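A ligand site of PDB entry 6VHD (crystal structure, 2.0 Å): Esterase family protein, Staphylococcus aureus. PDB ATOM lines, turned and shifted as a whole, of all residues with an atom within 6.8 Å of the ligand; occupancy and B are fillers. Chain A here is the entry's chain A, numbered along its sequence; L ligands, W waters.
A carbon (C12) of the ligand is covalently linked to the side-chain hydroxyl (OG) of Ser 123 (1.4 Å).
The backbone NH (N) of Met 124 is in hydrogen-bond range of an oxygen (O1) of the ligand (2.9 Å).
N of Leu 50 lies within hydrogen-bond range of O1 of the ligand.
A ring nitrogen (NE2) of His 236 sits at hydrogen-bond distance from the side-chain hydroxyl of Ser 123 (3.3 Å).
O of Ser 147 lies close to N of Ser 123 (3.3 Å).
A ring nitrogen (ND1) of His 236 is in hydrogen-bond range of the side-chain carboxylate (OD2) of Asp 207 (2.8 Å).
The backbone NH (N) of Leu 209 is in hydrogen-bond range of the side-chain carboxylate (OD1) of Asp 207.
The backbone NH (N) of Gly 49 lies close to a ring nitrogen (NE2) of His 122, at 3.5 Å.
CA of Gly 49 touches O1 of the ligand, at 3.9 Å.
Val 149 touches the ligand.
O of Asn 154 touches C6 of the ligand, at 3.5 Å.
Leu 155 touches the ligand.
Leu 158 touches the ligand.
Trp 160 touches the ligand (CE3 to C10, 3.7 Å).
Phe 208 touches the ligand.
Leu 209 touches the ligand (CD2 to C3, 3.6 Å).
NE2 of His 236 touches C5 of the ligand, at 3.1 Å.
Hydrophobic or aromatic side chains within 4 Å of the ligand: Leu 50, Met 124, Val 149, Leu 155, Leu 158, Trp 160, Phe 208, Leu 209 and His 236.
Within 4 Å of the ligand: Gly 49, Leu 50, Ser 123, Met 124, Val 149, Asn 154, Leu 155, Leu 158, Trp 160, Phe 208, Leu 209 and His 236.
Water W1 lies within hydrogen-bond range of a ring nitrogen (NE2) of His 236 (3.1 Å), an oxygen (O1) of the ligand (3.2 Å) and the side-chain hydroxyl of Ser 123 (3.2 Å).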
ATOM      1  N   HIS A  48     -35.447  -6.667 -29.556  1.00  0.00           N
ATOM      2  CA  HIS A  48     -34.460  -7.001 -30.571  1.00  0.00           C
ATOM      3  C   HIS A  48     -33.017  -6.744 -30.087  1.00  0.00           C
ATOM      4  O   HIS A  48     -32.769  -6.049 -29.092  1.00  0.00           O
ATOM      5  CB  HIS A  48     -34.726  -6.212 -31.846  1.00  0.00           C
ATOM      6  CG  HIS A  48     -34.537  -4.732 -31.676  1.00  0.00           C
ATOM      7  ND1 HIS A  48     -33.290  -4.141 -31.602  1.00  0.00           N
ATOM      8  CD2 HIS A  48     -35.427  -3.716 -31.569  1.00  0.00           C
ATOM      9  CE1 HIS A  48     -33.426  -2.841 -31.441  1.00  0.00           C
ATOM     10  NE2 HIS A  48     -34.715  -2.555 -31.412  1.00  0.00           N
ATOM     11  N   GLY A  49     -32.055  -7.314 -30.817  1.00  0.00           N
ATOM     12  CA  GLY A  49     -30.648  -7.113 -30.558  1.00  0.00           C
ATOM     13  C   GLY A  49     -30.081  -5.906 -31.302  1.00  0.00           C
ATOM     14  O   GLY A  49     -30.777  -5.200 -32.037  1.00  0.00           O
ATOM     15  N   LEU A  50     -28.781  -5.687 -31.122  1.00  0.00           N
ATOM     16  CA  LEU A  50     -28.125  -4.549 -31.753  1.00  0.00           C
ATOM     17  C   LEU A  50     -28.119  -4.729 -33.259  1.00  0.00           C
ATOM     18  O   LEU A  50     -27.815  -5.806 -33.770  1.00  0.00           O
ATOM     19  CB  LEU A  50     -26.692  -4.396 -31.239  1.00  0.00           C
ATOM     20  CG  LEU A  50     -25.847  -3.218 -31.763  1.00  0.00           C
ATOM     21  CD1 LEU A  50     -26.484  -1.914 -31.345  1.00  0.00           C
ATOM     22  CD2 LEU A  50     -24.421  -3.291 -31.210  1.00  0.00           C
ATOM     23  N   SER A  51     -28.450  -3.653 -33.978  1.00  0.00           N
ATOM     24  CA  SER A  51     -28.530  -3.554 -35.429  1.00  0.00           C
ATOM     25  C   SER A  51     -29.873  -4.091 -35.968  1.00  0.00           C
ATOM     26  O   SER A  51     -30.155  -3.898 -37.151  1.00  0.00           O
ATOM     27  CB  SER A  51     -27.374  -4.232 -36.171  1.00  0.00           C
ATOM     28  OG  SER A  51     -27.568  -5.640 -36.235  1.00  0.00           O
ATOM     29  N   HIS A 122     -33.147 -11.005 -27.402  1.00  0.00           N
ATOM     30  CA  HIS A 122     -31.839 -11.602 -27.646  1.00  0.00           C
ATOM     31  C   HIS A 122     -30.711 -10.555 -27.695  1.00  0.00           C
ATOM     32  O   HIS A 122     -30.916  -9.417 -28.127  1.00  0.00           O
ATOM     33  CB  HIS A 122     -31.851 -12.446 -28.949  1.00  0.00           C
ATOM     34  CG  HIS A 122     -31.903 -11.634 -30.206  1.00  0.00           C
ATOM     35  ND1 HIS A 122     -33.088 -11.190 -30.761  1.00  0.00           N
ATOM     36  CD2 HIS A 122     -30.918 -11.208 -31.027  1.00  0.00           C
ATOM     37  CE1 HIS A 122     -32.824 -10.526 -31.870  1.00  0.00           C
ATOM     38  NE2 HIS A 122     -31.514 -10.509 -32.055  1.00  0.00           N
ATOM     39  N   SER A 123     -29.509 -10.981 -27.248  1.00  0.00           N
ATOM     40  CA  SER A 123     -28.279 -10.185 -27.238  1.00  0.00           C
ATOM     41  C   SER A 123     -28.494  -8.896 -26.441  1.00  0.00           C
ATOM     42  O   SER A 123     -28.737  -8.985 -25.226  1.00  0.00           O
ATOM     43  CB  SER A 123     -27.806 -10.000 -28.697  1.00  0.00           C
ATOM     44  OG  SER A 123     -26.511  -9.405 -28.784  1.00  0.00           O
ATOM     45  N   MET A 124     -28.389  -7.704 -27.035  1.00  0.00           N
ATOM     46  CA  MET A 124     -28.765  -6.463 -26.359  1.00  0.00           C
ATOM     47  C   MET A 124     -30.195  -6.533 -25.810  1.00  0.00           C
ATOM     48  O   MET A 124     -30.495  -5.930 -24.768  1.00  0.00           O
ATOM     49  CB  MET A 124     -28.626  -5.277 -27.333  1.00  0.00           C
ATOM     50  CG  MET A 124     -28.816  -3.876 -26.767  1.00  0.00           C
ATOM     51  SD  MET A 124     -28.834  -2.605 -28.098  1.00  0.00           S
ATOM     52  CE  MET A 124     -30.506  -2.855 -28.752  1.00  0.00           C
ATOM     53  N   GLY A 125     -31.075  -7.245 -26.510  1.00  0.00           N
ATOM     54  CA  GLY A 125     -32.438  -7.448 -26.022  1.00  0.00           C
ATOM     55  C   GLY A 125     -32.528  -8.437 -24.874  1.00  0.00           C
ATOM     56  O   GLY A 125     -33.469  -8.374 -24.090  1.00  0.00           O
ATOM     57  N   SER A 147     -29.326 -15.621 -25.504  1.00  0.00           N
ATOM     58  CA  SER A 147     -27.974 -15.218 -25.852  1.00  0.00           C
ATOM     59  C   SER A 147     -27.661 -13.825 -25.293  1.00  0.00           C
ATOM     60  O   SER A 147     -27.169 -12.936 -25.991  1.00  0.00           O
ATOM     61  CB  SER A 147     -27.780 -15.259 -27.368  1.00  0.00           C
ATOM     62  OG  SER A 147     -28.329 -16.455 -27.894  1.00  0.00           O
ATOM     63  N   ALA A 148     -27.980 -13.637 -24.013  1.00  0.00           N
ATOM     64  CA  ALA A 148     -27.938 -12.309 -23.407  1.00  0.00           C
ATOM     65  C   ALA A 148     -26.521 -11.869 -23.078  1.00  0.00           C
ATOM     66  O   ALA A 148     -25.590 -12.669 -22.935  1.00  0.00           O
ATOM     67  CB  ALA A 148     -28.766 -12.290 -22.131  1.00  0.00           C
ATOM     68  N   VAL A 149     -26.369 -10.552 -22.946  1.00  0.00           N
ATOM     69  CA  VAL A 149     -25.185  -9.938 -22.356  1.00  0.00           C
ATOM     70  C   VAL A 149     -25.532  -9.667 -20.904  1.00  0.00           C
ATOM     71  O   VAL A 149     -26.449  -8.881 -20.617  1.00  0.00           O
ATOM     72  CB  VAL A 149     -24.782  -8.640 -23.078  1.00  0.00           C
ATOM     73  CG1 VAL A 149     -23.389  -8.231 -22.640  1.00  0.00           C
ATOM     74  CG2 VAL A 149     -24.874  -8.805 -24.570  1.00  0.00           C
ATOM     75  N   GLU A 151     -22.659  -9.389 -18.502  1.00  0.00           N
ATOM     76  CA  GLU A 151     -21.571  -8.503 -18.107  1.00  0.00           C
ATOM     77  C   GLU A 151     -21.625  -7.285 -19.018  1.00  0.00           C
ATOM     78  O   GLU A 151     -21.167  -7.321 -20.158  1.00  0.00           O
ATOM     79  CB  GLU A 151     -20.223  -9.191 -18.180  1.00  0.00           C
ATOM     80  CG  GLU A 151     -19.071  -8.275 -17.787  1.00  0.00           C
ATOM     81  CD  GLU A 151     -19.427  -7.375 -16.608  1.00  0.00           C
ATOM     82  OE1 GLU A 151     -19.755  -6.169 -16.830  1.00  0.00           O
ATOM     83  OE2 GLU A 151     -19.384  -7.870 -15.453  1.00  0.00           O
ATOM     84  N   ALA A 152     -22.198  -6.190 -18.500  1.00  0.00           N
ATOM     85  CA  ALA A 152     -22.515  -5.031 -19.341  1.00  0.00           C
ATOM     86  C   ALA A 152     -21.273  -4.415 -19.972  1.00  0.00           C
ATOM     87  O   ALA A 152     -21.380  -3.768 -21.027  1.00  0.00           O
ATOM     88  CB  ALA A 152     -23.271  -3.988 -18.528  1.00  0.00           C
ATOM     89  N   GLN A 153     -20.087  -4.576 -19.355  1.00  0.00           N
ATOM     90  CA  GLN A 153     -18.912  -3.926 -19.935  1.00  0.00           C
ATOM     91  C   GLN A 153     -18.528  -4.513 -21.288  1.00  0.00           C
ATOM     92  O   GLN A 153     -17.963  -3.812 -22.132  1.00  0.00           O
ATOM     93  CB  GLN A 153     -17.741  -4.044 -18.958  1.00  0.00           C
ATOM     94  CG  GLN A 153     -16.549  -3.167 -19.322  1.00  0.00           C
ATOM     95  CD  GLN A 153     -16.846  -1.700 -19.110  1.00  0.00           C
ATOM     96  OE1 GLN A 153     -17.437  -1.307 -18.103  1.00  0.00           O
ATOM     97  NE2 GLN A 153     -16.451  -0.872 -20.080  1.00  0.00           N
ATOM     98  N   ASN A 154     -18.892  -5.777 -21.536  1.00  0.00           N
ATOM     99  CA  ASN A 154     -18.639  -6.377 -22.841  1.00  0.00           C
ATOM    100  C   ASN A 154     -19.510  -5.747 -23.937  1.00  0.00           C
ATOM    101  O   ASN A 154     -19.100  -5.679 -25.103  1.00  0.00           O
ATOM    102  CB  ASN A 154     -18.837  -7.877 -22.747  1.00  0.00           C
ATOM    103  CG  ASN A 154     -17.838  -8.514 -21.802  1.00  0.00           C
ATOM    104  OD1 ASN A 154     -16.760  -7.975 -21.581  1.00  0.00           O
ATOM    105  ND2 ASN A 154     -18.195  -9.661 -21.234  1.00  0.00           N
ATOM    106  N   LEU A 155     -20.743  -5.350 -23.600  1.00  0.00           N
ATOM    107  CA  LEU A 155     -21.554  -4.617 -24.576  1.00  0.00           C
ATOM    108  C   LEU A 155     -20.991  -3.219 -24.808  1.00  0.00           C
ATOM    109  O   LEU A 155     -20.783  -2.803 -25.948  1.00  0.00           O
ATOM    110  CB  LEU A 155     -23.006  -4.535 -24.075  1.00  0.00           C
ATOM    111  CG  LEU A 155     -24.092  -3.885 -24.960  1.00  0.00           C
ATOM    112  CD1 LEU A 155     -23.928  -4.176 -26.462  1.00  0.00           C
ATOM    113  CD2 LEU A 155     -25.481  -4.294 -24.486  1.00  0.00           C
ATOM    114  N   MET A 156     -20.679  -2.501 -23.729  1.00  0.00           N
ATOM    115  CA  MET A 156     -20.215  -1.121 -23.892  1.00  0.00           C
ATOM    116  C   MET A 156     -18.890  -1.042 -24.641  1.00  0.00           C
ATOM    117  O   MET A 156     -18.642  -0.053 -25.346  1.00  0.00           O
ATOM    118  CB  MET A 156     -20.108  -0.443 -22.517  1.00  0.00           C
ATOM    119  CG  MET A 156     -21.425  -0.359 -21.727  1.00  0.00           C
ATOM    120  SD  MET A 156     -22.840   0.065 -22.758  1.00  0.00           S
ATOM    121  CE  MET A 156     -24.195  -0.128 -21.603  1.00  0.00           C
ATOM    122  N   LEU A 158     -17.787  -3.160 -27.056  1.00  0.00           N
ATOM    123  CA  LEU A 158     -17.851  -3.771 -28.417  1.00  0.00           C
ATOM    124  C   LEU A 158     -17.576  -2.701 -29.472  1.00  0.00           C
ATOM    125  O   LEU A 158     -18.035  -1.589 -29.314  1.00  0.00           O
ATOM    126  CB  LEU A 158     -19.263  -4.355 -28.574  1.00  0.00           C
ATOM    127  CG  LEU A 158     -19.495  -5.223 -29.803  1.00  0.00           C
ATOM    128  CD1 LEU A 158     -18.576  -6.436 -29.789  1.00  0.00           C
ATOM    129  CD2 LEU A 158     -20.930  -5.656 -29.880  1.00  0.00           C
ATOM    130  N   TRP A 160     -18.768  -2.477 -32.476  1.00  0.00           N
ATOM    131  CA  TRP A 160     -19.818  -2.666 -33.513  1.00  0.00           C
ATOM    132  C   TRP A 160     -19.960  -1.419 -34.377  1.00  0.00           C
ATOM    133  O   TRP A 160     -19.881  -0.309 -33.870  1.00  0.00           O
ATOM    134  CB  TRP A 160     -21.152  -3.041 -32.843  1.00  0.00           C
ATOM    135  CG  TRP A 160     -22.226  -3.335 -33.848  1.00  0.00           C
ATOM    136  CD1 TRP A 160     -23.124  -2.452 -34.371  1.00  0.00           C
ATOM    137  CD2 TRP A 160     -22.447  -4.574 -34.530  1.00  0.00           C
ATOM    138  NE1 TRP A 160     -23.901  -3.062 -35.309  1.00  0.00           N
ATOM    139  CE2 TRP A 160     -23.512  -4.365 -35.424  1.00  0.00           C
ATOM    140  CE3 TRP A 160     -21.843  -5.828 -34.466  1.00  0.00           C
ATOM    141  CZ2 TRP A 160     -23.999  -5.385 -36.235  1.00  0.00           C
ATOM    142  CZ3 TRP A 160     -22.335  -6.835 -35.260  1.00  0.00           C
ATOM    143  CH2 TRP A 160     -23.397  -6.616 -36.125  1.00  0.00           C
ATOM    144  N   ASP A 207     -21.965 -20.063 -29.032  1.00  0.00           N
ATOM    145  CA  ASP A 207     -22.107 -18.595 -28.981  1.00  0.00           C
ATOM    146  C   ASP A 207     -20.909 -18.004 -28.246  1.00  0.00           C
ATOM    147  O   ASP A 207     -20.564 -18.523 -27.205  1.00  0.00           O
ATOM    148  CB  ASP A 207     -23.408 -18.229 -28.258  1.00  0.00           C
ATOM    149  CG  ASP A 207     -23.833 -16.793 -28.421  1.00  0.00           C
ATOM    150  OD1 ASP A 207     -22.987 -15.932 -28.332  1.00  0.00           O
ATOM    151  OD2 ASP A 207     -25.013 -16.567 -28.671  1.00  0.00           O
ATOM    152  N   PHE A 208     -20.397 -16.861 -28.678  1.00  0.00           N
ATOM    153  CA  PHE A 208     -19.276 -16.177 -27.993  1.00  0.00           C
ATOM    154  C   PHE A 208     -19.680 -15.709 -26.578  1.00  0.00           C
ATOM    155  O   PHE A 208     -18.789 -15.527 -25.787  1.00  0.00           O
ATOM    156  CB  PHE A 208     -18.667 -15.043 -28.817  1.00  0.00           C
ATOM    157  CG  PHE A 208     -19.672 -14.303 -29.664  1.00  0.00           C
ATOM    158  CD1 PHE A 208     -20.194 -13.095 -29.251  1.00  0.00           C
ATOM    159  CD2 PHE A 208     -20.100 -14.835 -30.867  1.00  0.00           C
ATOM    160  CE1 PHE A 208     -21.121 -12.421 -30.031  1.00  0.00           C
ATOM    161  CE2 PHE A 208     -21.026 -14.162 -31.647  1.00  0.00           C
ATOM    162  CZ  PHE A 208     -21.526 -12.956 -31.224  1.00  0.00           C
ATOM    163  N   LEU A 209     -20.966 -15.453 -26.314  1.00  0.00           N
ATOM    164  CA  LEU A 209     -21.484 -15.031 -24.990  1.00  0.00           C
ATOM    165  C   LEU A 209     -21.803 -16.243 -24.107  1.00  0.00           C
ATOM    166  O   LEU A 209     -22.365 -16.048 -23.060  1.00  0.00           O
ATOM    167  CB  LEU A 209     -22.744 -14.192 -25.220  1.00  0.00           C
ATOM    168  CG  LEU A 209     -22.535 -12.846 -25.891  1.00  0.00           C
ATOM    169  CD1 LEU A 209     -23.858 -12.153 -26.135  1.00  0.00           C
ATOM    170  CD2 LEU A 209     -21.631 -11.969 -25.053  1.00  0.00           C
ATOM    171  N   ASP A 212     -20.299 -15.945 -20.731  1.00  0.00           N
ATOM    172  CA  ASP A 212     -21.020 -14.847 -20.048  1.00  0.00           C
ATOM    173  C   ASP A 212     -22.313 -15.396 -19.422  1.00  0.00           C
ATOM    174  O   ASP A 212     -22.586 -15.041 -18.292  1.00  0.00           O
ATOM    175  CB  ASP A 212     -21.170 -13.680 -21.010  1.00  0.00           C
ATOM    176  CG  ASP A 212     -21.991 -12.536 -20.465  1.00  0.00           C
ATOM    177  OD1 ASP A 212     -21.492 -11.432 -20.463  1.00  0.00           O
ATOM    178  OD2 ASP A 212     -23.135 -12.781 -20.072  1.00  0.00           O
ATOM    179  N   HIS A 236     -24.705 -17.473 -32.460  1.00  0.00           N
ATOM    180  CA  HIS A 236     -25.314 -16.179 -32.201  1.00  0.00           C
ATOM    181  C   HIS A 236     -26.002 -15.662 -33.476  1.00  0.00           C
ATOM    182  O   HIS A 236     -25.529 -14.742 -34.134  1.00  0.00           O
ATOM    183  CB  HIS A 236     -24.240 -15.210 -31.717  1.00  0.00           C
ATOM    184  CG  HIS A 236     -24.802 -13.991 -31.062  1.00  0.00           C
ATOM    185  ND1 HIS A 236     -25.062 -13.933 -29.710  1.00  0.00           N
ATOM    186  CD2 HIS A 236     -25.186 -12.805 -31.573  1.00  0.00           C
ATOM    187  CE1 HIS A 236     -25.559 -12.752 -29.413  1.00  0.00           C
ATOM    188  NE2 HIS A 236     -25.660 -12.052 -30.531  1.00  0.00           N
ATOM    189  N   TRP A 241     -32.139 -18.246 -32.833  1.00  0.00           N
ATOM    190  CA  TRP A 241     -33.220 -17.540 -32.130  1.00  0.00           C
ATOM    191  C   TRP A 241     -34.594 -17.988 -32.602  1.00  0.00           C
ATOM    192  O   TRP A 241     -35.547 -17.990 -31.818  1.00  0.00           O
ATOM    193  CB  TRP A 241     -33.046 -16.013 -32.252  1.00  0.00           C
ATOM    194  CG  TRP A 241     -31.745 -15.567 -31.581  1.00  0.00           C
ATOM    195  CD1 TRP A 241     -31.264 -16.003 -30.372  1.00  0.00           C
ATOM    196  CD2 TRP A 241     -30.753 -14.663 -32.096  1.00  0.00           C
ATOM    197  NE1 TRP A 241     -30.041 -15.425 -30.104  1.00  0.00           N
ATOM    198  CE2 TRP A 241     -29.703 -14.599 -31.149  1.00  0.00           C
ATOM    199  CE3 TRP A 241     -30.647 -13.895 -33.266  1.00  0.00           C
ATOM    200  CZ2 TRP A 241     -28.577 -13.801 -31.333  1.00  0.00           C
ATOM    201  CZ3 TRP A 241     -29.528 -13.110 -33.448  1.00  0.00           C
ATOM    202  CH2 TRP A 241     -28.497 -13.066 -32.493  1.00  0.00           C
HETATM  203  C1  LIG L   1     -22.457  -8.548 -28.301  1.00  0.00           C
HETATM  204  C2  LIG L   1     -23.293  -8.509 -29.577  1.00  0.00           C
HETATM  205  C3  LIG L   1     -20.460  -9.289 -27.189  1.00  0.00           C
HETATM  206  C4  LIG L   1     -23.600  -9.323 -31.785  1.00  0.00           C
HETATM  207  C5  LIG L   1     -23.542  -9.807 -30.329  1.00  0.00           C
HETATM  208  C6  LIG L   1     -20.832  -8.572 -26.061  1.00  0.00           C
HETATM  209  C7  LIG L   1     -22.011  -7.840 -26.065  1.00  0.00           C
HETATM  210  C8  LIG L   1     -22.817  -7.815 -27.186  1.00  0.00           C
HETATM  211  C9  LIG L   1     -21.266  -9.264 -28.311  1.00  0.00           C
HETATM  212  C10 LIG L   1     -23.664  -7.774 -31.932  1.00  0.00           C
HETATM  213  C11 LIG L   1     -24.559  -7.045 -30.917  1.00  0.00           C
HETATM  214  N1  LIG L   1     -24.520  -7.732 -29.632  1.00  0.00           N
HETATM  215  C12 LIG L   1     -25.831  -8.310 -29.264  1.00  0.00           C
HETATM  216  O1  LIG L   1     -26.917  -7.548 -29.547  1.00  0.00           O
HETATM  217  O   HOH W   1     -27.013  -9.665 -31.945  1.00  0.00           O
